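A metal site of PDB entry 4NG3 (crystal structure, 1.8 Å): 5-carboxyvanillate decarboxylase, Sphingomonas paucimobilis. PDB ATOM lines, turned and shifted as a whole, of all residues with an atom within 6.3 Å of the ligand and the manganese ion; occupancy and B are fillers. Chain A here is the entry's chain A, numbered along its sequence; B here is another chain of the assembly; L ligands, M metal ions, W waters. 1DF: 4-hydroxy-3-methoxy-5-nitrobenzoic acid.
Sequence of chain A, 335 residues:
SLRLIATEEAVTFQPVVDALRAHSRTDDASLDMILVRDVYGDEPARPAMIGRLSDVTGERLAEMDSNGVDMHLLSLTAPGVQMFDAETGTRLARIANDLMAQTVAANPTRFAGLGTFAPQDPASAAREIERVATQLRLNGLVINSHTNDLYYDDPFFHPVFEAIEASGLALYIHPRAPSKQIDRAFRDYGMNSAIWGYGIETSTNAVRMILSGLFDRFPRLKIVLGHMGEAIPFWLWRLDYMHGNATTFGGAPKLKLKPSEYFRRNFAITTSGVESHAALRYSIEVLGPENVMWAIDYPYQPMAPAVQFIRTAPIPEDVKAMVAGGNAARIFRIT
Three residues have an atom within 4 Å of the manganese ion: Glu 8, His 174 and Asp 297.
Along chain A the residues within 4 Å of the manganese ion span positions 8 to 297.
The nearest printed residue that does not touch the manganese ion is His 227 (4.3 Å).
Residues that only touch the ligand: Ala 78, Leu 35, Thr 77, Ser 193, Asn 245 of chain B, Ala 194, Tyr 198 and Met 242 of chain B.
Hydrophobic or aromatic side chains within 4 Å of the ligand: Leu 35, Ala 78, His 174, Ala 194, Tyr 198, His 227, Tyr 300 and Met 242 of chain B.
Within 4 Å of the ligand: Glu 8, Leu 35, Arg 46, Thr 77, Ala 78, His 174, Ser 193, Ala 194, Tyr 198, His 227, Asp 297, Tyr 300, Arg 238 of chain B, Met 242 of chain B and Asn 245 of chain B.
Along chain A the residues within 4 Å of the ligand span positions 8 to 300.
The manganese ion is bound by an oxygen (O11) of the ligand (1.9 Å), an oxygen (O3) of the ligand (2.1 Å), the side-chain carboxylate (OE2) of Glu 8 (2.2 Å), a ring nitrogen (NE2) of His 174 (2.2 Å), water W3 (2.2 Å) and the side-chain carboxylate (OD1) of Asp 297 (2.3 Å).
The guanidinium group (NH1) of Arg 46 lies within salt-bridge range of an oxygen (O2) of the ligand (2.8 Å).
The side-chain hydroxyl (OH) of Tyr 300 lies close to an oxygen (OM) of the ligand.
An oxygen (O22) of the ligand is in hydrogen-bond range of a ring nitrogen (NE2) of His 227.
O22 of the ligand is in hydrogen-bond range of NH2 of Arg 238 of chain B (3.0 Å).
The side-chain carboxylate (OD2) of Asp 297 lies within hydrogen-bond range of a ring nitrogen (NE2) of His 227, 3.1 Å away.
The side-chain sulfur (SD) of Met 242 of chain B lies within hydrogen-bond range of the side-chain amide nitrogen (ND2) of Asn 245 of chain B (3.5 Å).
A ring nitrogen (NE2) of His 227 lies close to the guanidinium group of Arg 238 of chain B (3.4 Å).
N of His 227 lies within hydrogen-bond range of OG of Ser 272 (2.9 Å).
A ring nitrogen (NE2) of His 227 lies close to the side-chain carboxylate of Glu 8 (3.3 Å).
The side-chain carboxylate (OE1) of Glu 8 lies within hydrogen-bond range of the side-chain hydroxyl (OG) of Ser 272, 2.6 Å away.
The guanidinium group (NE) of Arg 238 of chain B sits at hydrogen-bond distance from the backbone carbonyl oxygen (O) of Ala 194.
The backbone carbonyl oxygen of Ser 193 is in hydrogen-bond range of the backbone NH of Tyr 198 (3.0 Å).
Water W4 lies within hydrogen-bond range of an oxygen (O1) of the ligand (2.6 Å), the side-chain amide nitrogen of Asn 245 of chain B (2.8 Å), the backbone carbonyl oxygen of Tyr 300 (2.9 Å) and the guanidinium group of Arg 46 (3.5 Å).
Water W6 lies within hydrogen-bond range of OH of Tyr 198, O2 of the ligand and OG of Ser 193.
Water W2 lies within hydrogen-bond range of an oxygen (O1) of the ligand (2.7 Å), the side-chain amide nitrogen (ND2) of Asn 245 of chain B (2.9 Å) and the side-chain hydroxyl (OG) of Ser 193 (3.0 Å).
Water W5 lies within hydrogen-bond range of the side-chain hydroxyl (OG1) of Thr 77 (2.7 Å), an oxygen (OM) of the ligand (3.0 Å) and the backbone NH (N) of Ala 78 (3.0 Å).
Water W1 lies within hydrogen-bond range of OD2 of Asp 297 (2.7 Å), NE2 of Gln 301 (2.8 Å), NH1 of Arg 238 of chain B (2.9 Å) and O22 of the ligand (3.0 Å).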
ATOM      1  N   GLU A   8      11.529 -30.442  18.191  1.00  0.00           N
ATOM      2  CA  GLU A   8      10.794 -29.696  19.221  1.00  0.00           C
ATOM      3  C   GLU A   8       9.334 -29.492  18.825  1.00  0.00           C
ATOM      4  O   GLU A   8       8.852 -28.368  18.718  1.00  0.00           O
ATOM      5  CB  GLU A   8      11.457 -28.340  19.545  1.00  0.00           C
ATOM      6  CG  GLU A   8      10.959 -27.719  20.863  1.00  0.00           C
ATOM      7  CD  GLU A   8      11.514 -26.314  21.103  1.00  0.00           C
ATOM      8  OE1 GLU A   8      12.752 -26.139  21.141  1.00  0.00           O
ATOM      9  OE2 GLU A   8      10.698 -25.374  21.244  1.00  0.00           O
ATOM     10  N   ALA A  10       5.475 -29.707  19.300  1.00  0.00           N
ATOM     11  CA  ALA A  10       4.533 -29.708  20.406  1.00  0.00           C
ATOM     12  C   ALA A  10       3.263 -30.471  20.083  1.00  0.00           C
ATOM     13  O   ALA A  10       2.782 -30.458  18.961  1.00  0.00           O
ATOM     14  CB  ALA A  10       4.209 -28.265  20.825  1.00  0.00           C
ATOM     15  N   LEU A  35      -0.237 -17.293  28.630  1.00  0.00           N
ATOM     16  CA  LEU A  35      -0.415 -18.340  27.631  1.00  0.00           C
ATOM     17  C   LEU A  35      -1.652 -19.186  27.930  1.00  0.00           C
ATOM     18  O   LEU A  35      -2.449 -19.479  27.032  1.00  0.00           O
ATOM     19  CB  LEU A  35       0.831 -19.248  27.600  1.00  0.00           C
ATOM     20  CG  LEU A  35       0.678 -20.578  26.867  1.00  0.00           C
ATOM     21  CD1 LEU A  35       0.619 -20.325  25.367  1.00  0.00           C
ATOM     22  CD2 LEU A  35       1.837 -21.527  27.211  1.00  0.00           C
ATOM     23  N   TYR A  40      -5.967 -21.865  26.379  1.00  0.00           N
ATOM     24  CA  TYR A  40      -6.852 -22.811  27.063  1.00  0.00           C
ATOM     25  C   TYR A  40      -8.046 -22.154  27.753  1.00  0.00           C
ATOM     26  O   TYR A  40      -8.877 -22.830  28.346  1.00  0.00           O
ATOM     27  CB  TYR A  40      -6.048 -23.651  28.066  1.00  0.00           C
ATOM     28  CG  TYR A  40      -4.883 -24.351  27.433  1.00  0.00           C
ATOM     29  CD1 TYR A  40      -5.042 -25.584  26.813  1.00  0.00           C
ATOM     30  CD2 TYR A  40      -3.618 -23.779  27.435  1.00  0.00           C
ATOM     31  CE1 TYR A  40      -3.982 -26.222  26.217  1.00  0.00           C
ATOM     32  CE2 TYR A  40      -2.544 -24.409  26.832  1.00  0.00           C
ATOM     33  CZ  TYR A  40      -2.734 -25.636  26.231  1.00  0.00           C
ATOM     34  OH  TYR A  40      -1.678 -26.284  25.631  1.00  0.00           O
ATOM     35  N   ARG A  46      -6.205 -17.026  21.143  1.00  0.00           N
ATOM     36  CA  ARG A  46      -5.618 -17.927  20.173  1.00  0.00           C
ATOM     37  C   ARG A  46      -6.455 -19.197  20.084  1.00  0.00           C
ATOM     38  O   ARG A  46      -6.001 -20.274  20.475  1.00  0.00           O
ATOM     39  CB  ARG A  46      -4.174 -18.254  20.583  1.00  0.00           C
ATOM     40  CG  ARG A  46      -3.297 -17.020  20.731  1.00  0.00           C
ATOM     41  CD  ARG A  46      -1.963 -17.342  21.380  1.00  0.00           C
ATOM     42  NE  ARG A  46      -0.996 -17.957  20.463  1.00  0.00           N
ATOM     43  CZ  ARG A  46       0.250 -18.271  20.797  1.00  0.00           C
ATOM     44  NH1 ARG A  46       0.681 -18.023  22.033  1.00  0.00           N
ATOM     45  NH2 ARG A  46       1.088 -18.829  19.922  1.00  0.00           N
ATOM     46  N   THR A  77       3.257 -30.026  25.170  1.00  0.00           N
ATOM     47  CA  THR A  77       3.576 -28.610  25.024  1.00  0.00           C
ATOM     48  C   THR A  77       3.697 -27.938  26.388  1.00  0.00           C
ATOM     49  O   THR A  77       3.089 -28.383  27.363  1.00  0.00           O
ATOM     50  CB  THR A  77       2.494 -27.895  24.200  1.00  0.00           C
ATOM     51  OG1 THR A  77       2.922 -26.564  23.886  1.00  0.00           O
ATOM     52  CG2 THR A  77       1.164 -27.832  24.968  1.00  0.00           C
ATOM     53  N   ALA A  78       4.487 -26.875  26.441  1.00  0.00           N
ATOM     54  CA  ALA A  78       4.586 -26.103  27.673  1.00  0.00           C
ATOM     55  C   ALA A  78       3.204 -25.585  28.034  1.00  0.00           C
ATOM     56  O   ALA A  78       2.409 -25.264  27.151  1.00  0.00           O
ATOM     57  CB  ALA A  78       5.576 -24.947  27.498  1.00  0.00           C
ATOM     58  N   PRO A  79       2.904 -25.500  29.345  1.00  0.00           N
ATOM     59  CA  PRO A  79       3.768 -25.741  30.503  1.00  0.00           C
ATOM     60  C   PRO A  79       3.713 -27.182  31.012  1.00  0.00           C
ATOM     61  O   PRO A  79       3.992 -27.435  32.205  1.00  0.00           O
ATOM     62  CB  PRO A  79       3.170 -24.807  31.554  1.00  0.00           C
ATOM     63  CG  PRO A  79       1.697 -24.856  31.249  1.00  0.00           C
ATOM     64  CD  PRO A  79       1.572 -25.018  29.754  1.00  0.00           C
ATOM     65  N   HIS A 174      12.674 -27.460  27.817  1.00  0.00           N
ATOM     66  CA  HIS A 174      11.937 -26.523  26.978  1.00  0.00           C
ATOM     67  C   HIS A 174      11.584 -25.276  27.797  1.00  0.00           C
ATOM     68  O   HIS A 174      11.541 -25.332  29.037  1.00  0.00           O
ATOM     69  CB  HIS A 174      10.682 -27.232  26.452  1.00  0.00           C
ATOM     70  CG  HIS A 174       9.860 -26.405  25.506  1.00  0.00           C
ATOM     71  ND1 HIS A 174       8.934 -25.487  25.931  1.00  0.00           N
ATOM     72  CD2 HIS A 174       9.827 -26.381  24.152  1.00  0.00           C
ATOM     73  CE1 HIS A 174       8.373 -24.906  24.883  1.00  0.00           C
ATOM     74  NE2 HIS A 174       8.893 -25.435  23.795  1.00  0.00           N
ATOM     75  N   PRO A 175      11.340 -24.140  27.136  1.00  0.00           N
ATOM     76  CA  PRO A 175      10.980 -22.965  27.943  1.00  0.00           C
ATOM     77  C   PRO A 175       9.584 -23.024  28.550  1.00  0.00           C
ATOM     78  O   PRO A 175       8.727 -23.806  28.119  1.00  0.00           O
ATOM     79  CB  PRO A 175      10.979 -21.828  26.915  1.00  0.00           C
ATOM     80  CG  PRO A 175      11.906 -22.275  25.852  1.00  0.00           C
ATOM     81  CD  PRO A 175      11.661 -23.762  25.734  1.00  0.00           C
ATOM     82  N   SER A 193       6.708 -14.185  26.671  1.00  0.00           N
ATOM     83  CA  SER A 193       6.688 -15.321  25.751  1.00  0.00           C
ATOM     84  C   SER A 193       8.010 -15.540  25.019  1.00  0.00           C
ATOM     85  O   SER A 193       9.085 -15.158  25.486  1.00  0.00           O
ATOM     86  CB  SER A 193       5.524 -15.125  24.761  1.00  0.00           C
ATOM     87  OG  SER A 193       5.272 -16.298  23.977  1.00  0.00           O
ATOM     88  N   ALA A 194       7.901 -16.171  23.849  1.00  0.00           N
ATOM     89  CA  ALA A 194       9.072 -16.559  23.058  1.00  0.00           C
ATOM     90  C   ALA A 194       9.963 -15.396  22.618  1.00  0.00           C
ATOM     91  O   ALA A 194      11.185 -15.572  22.423  1.00  0.00           O
ATOM     92  CB  ALA A 194       8.624 -17.346  21.837  1.00  0.00           C
ATOM     93  N   TYR A 198      11.056 -16.437  27.397  1.00  0.00           N
ATOM     94  CA  TYR A 198      11.345 -17.874  27.322  1.00  0.00           C
ATOM     95  C   TYR A 198      12.852 -18.136  27.349  1.00  0.00           C
ATOM     96  O   TYR A 198      13.318 -19.033  28.048  1.00  0.00           O
ATOM     97  CB  TYR A 198      10.738 -18.492  26.047  1.00  0.00           C
ATOM     98  CG  TYR A 198       9.260 -18.837  26.148  1.00  0.00           C
ATOM     99  CD1 TYR A 198       8.500 -18.428  27.232  1.00  0.00           C
ATOM    100  CD2 TYR A 198       8.642 -19.608  25.163  1.00  0.00           C
ATOM    101  CE1 TYR A 198       7.146 -18.757  27.343  1.00  0.00           C
ATOM    102  CE2 TYR A 198       7.287 -19.941  25.252  1.00  0.00           C
ATOM    103  CZ  TYR A 198       6.548 -19.506  26.336  1.00  0.00           C
ATOM    104  OH  TYR A 198       5.208 -19.827  26.440  1.00  0.00           O
ATOM    105  N   HIS A 227      16.026 -23.272  20.590  1.00  0.00           N
ATOM    106  CA  HIS A 227      16.254 -21.846  20.320  1.00  0.00           C
ATOM    107  C   HIS A 227      17.741 -21.503  20.283  1.00  0.00           C
ATOM    108  O   HIS A 227      18.200 -20.524  20.878  1.00  0.00           O
ATOM    109  CB  HIS A 227      15.450 -21.005  21.316  1.00  0.00           C
ATOM    110  CG  HIS A 227      14.088 -21.569  21.524  1.00  0.00           C
ATOM    111  ND1 HIS A 227      13.692 -22.177  22.700  1.00  0.00           N
ATOM    112  CD2 HIS A 227      13.047 -21.715  20.669  1.00  0.00           C
ATOM    113  CE1 HIS A 227      12.466 -22.629  22.571  1.00  0.00           C
ATOM    114  NE2 HIS A 227      12.041 -22.367  21.351  1.00  0.00           N
ATOM    115  N   SER A 272      15.274 -24.641  16.884  1.00  0.00           N
ATOM    116  CA  SER A 272      13.877 -24.201  16.935  1.00  0.00           C
ATOM    117  C   SER A 272      13.754 -22.696  17.052  1.00  0.00           C
ATOM    118  O   SER A 272      14.368 -22.077  17.928  1.00  0.00           O
ATOM    119  CB  SER A 272      13.145 -24.874  18.089  1.00  0.00           C
ATOM    120  OG  SER A 272      13.864 -24.715  19.294  1.00  0.00           O
ATOM    121  N   GLY A 273      12.994 -22.096  16.141  1.00  0.00           N
ATOM    122  CA  GLY A 273      12.712 -20.669  16.203  1.00  0.00           C
ATOM    123  C   GLY A 273      13.899 -19.756  15.960  1.00  0.00           C
ATOM    124  O   GLY A 273      13.801 -18.541  16.172  1.00  0.00           O
ATOM    125  N   ASP A 297       9.573 -26.423  15.775  1.00  0.00           N
ATOM    126  CA  ASP A 297       8.744 -25.780  16.814  1.00  0.00           C
ATOM    127  C   ASP A 297       7.277 -25.652  16.352  1.00  0.00           C
ATOM    128  O   ASP A 297       6.581 -24.695  16.703  1.00  0.00           O
ATOM    129  CB  ASP A 297       9.309 -24.398  17.206  1.00  0.00           C
ATOM    130  CG  ASP A 297       9.234 -24.114  18.701  1.00  0.00           C
ATOM    131  OD1 ASP A 297       8.418 -24.745  19.404  1.00  0.00           O
ATOM    132  OD2 ASP A 297      10.006 -23.244  19.168  1.00  0.00           O
ATOM    133  N   TYR A 300       3.818 -23.742  16.757  1.00  0.00           N
ATOM    134  CA  TYR A 300       4.111 -22.344  17.076  1.00  0.00           C
ATOM    135  C   TYR A 300       4.906 -21.674  15.961  1.00  0.00           C
ATOM    136  O   TYR A 300       4.927 -20.440  15.859  1.00  0.00           O
ATOM    137  CB  TYR A 300       4.820 -22.231  18.424  1.00  0.00           C
ATOM    138  CG  TYR A 300       4.018 -22.864  19.539  1.00  0.00           C
ATOM    139  CD1 TYR A 300       2.838 -22.264  19.992  1.00  0.00           C
ATOM    140  CD2 TYR A 300       4.407 -24.071  20.114  1.00  0.00           C
ATOM    141  CE1 TYR A 300       2.091 -22.845  20.993  1.00  0.00           C
ATOM    142  CE2 TYR A 300       3.655 -24.663  21.121  1.00  0.00           C
ATOM    143  CZ  TYR A 300       2.499 -24.032  21.555  1.00  0.00           C
ATOM    144  OH  TYR A 300       1.737 -24.593  22.549  1.00  0.00           O
ATOM    145  N   GLN A 301       5.569 -22.485  15.134  1.00  0.00           N
ATOM    146  CA  GLN A 301       6.233 -22.019  13.910  1.00  0.00           C
ATOM    147  C   GLN A 301       5.757 -22.901  12.763  1.00  0.00           C
ATOM    148  O   GLN A 301       5.466 -24.079  12.972  1.00  0.00           O
ATOM    149  CB  GLN A 301       7.754 -22.188  14.009  1.00  0.00           C
ATOM    150  CG  GLN A 301       8.417 -21.458  15.156  1.00  0.00           C
ATOM    151  CD  GLN A 301       9.130 -20.201  14.710  1.00  0.00           C
ATOM    152  OE1 GLN A 301       9.245 -19.929  13.513  1.00  0.00           O
ATOM    153  NE2 GLN A 301       9.606 -19.436  15.675  1.00  0.00           N
ATOM    154  N   ARG B 238      14.929 -14.246  16.151  1.00  0.00           N
ATOM    155  CA  ARG B 238      13.799 -14.604  16.999  1.00  0.00           C
ATOM    156  C   ARG B 238      13.039 -13.367  17.457  1.00  0.00           C
ATOM    157  O   ARG B 238      11.796 -13.360  17.483  1.00  0.00           O
ATOM    158  CB  ARG B 238      14.291 -15.412  18.191  1.00  0.00           C
ATOM    159  CG  ARG B 238      13.204 -16.013  19.077  1.00  0.00           C
ATOM    160  CD  ARG B 238      13.743 -17.306  19.636  1.00  0.00           C
ATOM    161  NE  ARG B 238      13.005 -17.856  20.763  1.00  0.00           N
ATOM    162  CZ  ARG B 238      11.903 -18.594  20.670  1.00  0.00           C
ATOM    163  NH1 ARG B 238      11.352 -18.845  19.480  1.00  0.00           N
ATOM    164  NH2 ARG B 238      11.350 -19.083  21.776  1.00  0.00           N
ATOM    165  N   MET B 242       9.088 -13.248  16.400  1.00  0.00           N
ATOM    166  CA  MET B 242       8.053 -13.271  17.412  1.00  0.00           C
ATOM    167  C   MET B 242       7.389 -11.911  17.635  1.00  0.00           C
ATOM    168  O   MET B 242       6.451 -11.804  18.426  1.00  0.00           O
ATOM    169  CB  MET B 242       8.610 -13.826  18.741  1.00  0.00           C
ATOM    170  CG  MET B 242       8.842 -15.322  18.736  1.00  0.00           C
ATOM    171  SD  MET B 242       7.298 -16.158  18.345  1.00  0.00           S
ATOM    172  CE  MET B 242       7.805 -17.887  18.286  1.00  0.00           C
ATOM    173  N   ASN B 245       3.476 -11.810  17.041  1.00  0.00           N
ATOM    174  CA  ASN B 245       2.726 -12.283  18.189  1.00  0.00           C
ATOM    175  C   ASN B 245       2.637 -11.226  19.292  1.00  0.00           C
ATOM    176  O   ASN B 245       1.587 -11.029  19.916  1.00  0.00           O
ATOM    177  CB  ASN B 245       3.346 -13.557  18.764  1.00  0.00           C
ATOM    178  CG  ASN B 245       3.134 -14.770  17.890  1.00  0.00           C
ATOM    179  OD1 ASN B 245       2.320 -14.751  16.957  1.00  0.00           O
ATOM    180  ND2 ASN B 245       3.836 -15.847  18.199  1.00  0.00           N
ATOM    181  N   PHE B 249      -1.243 -10.347  20.143  1.00  0.00           N
ATOM    182  CA  PHE B 249      -1.938 -10.702  21.376  1.00  0.00           C
ATOM    183  C   PHE B 249      -1.162 -10.338  22.639  1.00  0.00           C
ATOM    184  O   PHE B 249      -1.687 -10.454  23.745  1.00  0.00           O
ATOM    185  CB  PHE B 249      -2.403 -12.170  21.381  1.00  0.00           C
ATOM    186  CG  PHE B 249      -1.352 -13.154  20.943  1.00  0.00           C
ATOM    187  CD1 PHE B 249      -0.423 -13.649  21.855  1.00  0.00           C
ATOM    188  CD2 PHE B 249      -1.313 -13.603  19.636  1.00  0.00           C
ATOM    189  CE1 PHE B 249       0.538 -14.560  21.469  1.00  0.00           C
ATOM    190  CE2 PHE B 249      -0.351 -14.511  19.241  1.00  0.00           C
ATOM    191  CZ  PHE B 249       0.582 -14.997  20.156  1.00  0.00           C
HETATM  192  C1  1DF L   1       5.104 -20.423  21.873  1.00  0.00           C
HETATM  193  CO1 1DF L   1       6.388 -20.649  21.366  1.00  0.00           C
HETATM  194  CO2 1DF L   1       4.517 -21.342  22.731  1.00  0.00           C
HETATM  195  CM1 1DF L   1       7.065 -21.814  21.729  1.00  0.00           C
HETATM  196  CM2 1DF L   1       5.200 -22.492  23.078  1.00  0.00           C
HETATM  197  OM  1DF L   1       4.668 -23.436  23.914  1.00  0.00           O
HETATM  198  CZ  1DF L   1       6.457 -22.732  22.574  1.00  0.00           C
HETATM  199  CC  1DF L   1       4.318 -19.205  21.543  1.00  0.00           C
HETATM  200  CV  1DF L   1       3.665 -23.133  24.829  1.00  0.00           C
HETATM  201  O1  1DF L   1       4.573 -18.538  20.513  1.00  0.00           O
HETATM  202  O2  1DF L   1       3.376 -18.863  22.309  1.00  0.00           O
HETATM  203  O3  1DF L   1       6.871 -24.034  22.619  1.00  0.00           O
HETATM  204  N   1DF L   1       8.476 -21.949  21.497  1.00  0.00           N
HETATM  205  O11 1DF L   1       9.105 -23.078  21.749  1.00  0.00           O
HETATM  206  O22 1DF L   1       9.153 -20.950  21.022  1.00  0.00           O
HETATM  207 MN    MN M   1       8.583 -24.861  21.653  1.00  0.00          MN
HETATM  208  O   HOH W   1       9.728 -20.754  18.117  1.00  0.00           O
HETATM  209  O   HOH W   2       4.364 -15.913  21.100  1.00  0.00           O
HETATM  210  O   HOH W   3       7.662 -26.831  21.111  1.00  0.00           O
HETATM  211  O   HOH W   4       3.948 -18.652  17.945  1.00  0.00           O
HETATM  212  O   HOH W   5       5.577 -26.261  23.677  1.00  0.00           O
HETATM  213  O   HOH W   6       3.708 -18.316  24.893  1.00  0.00           O
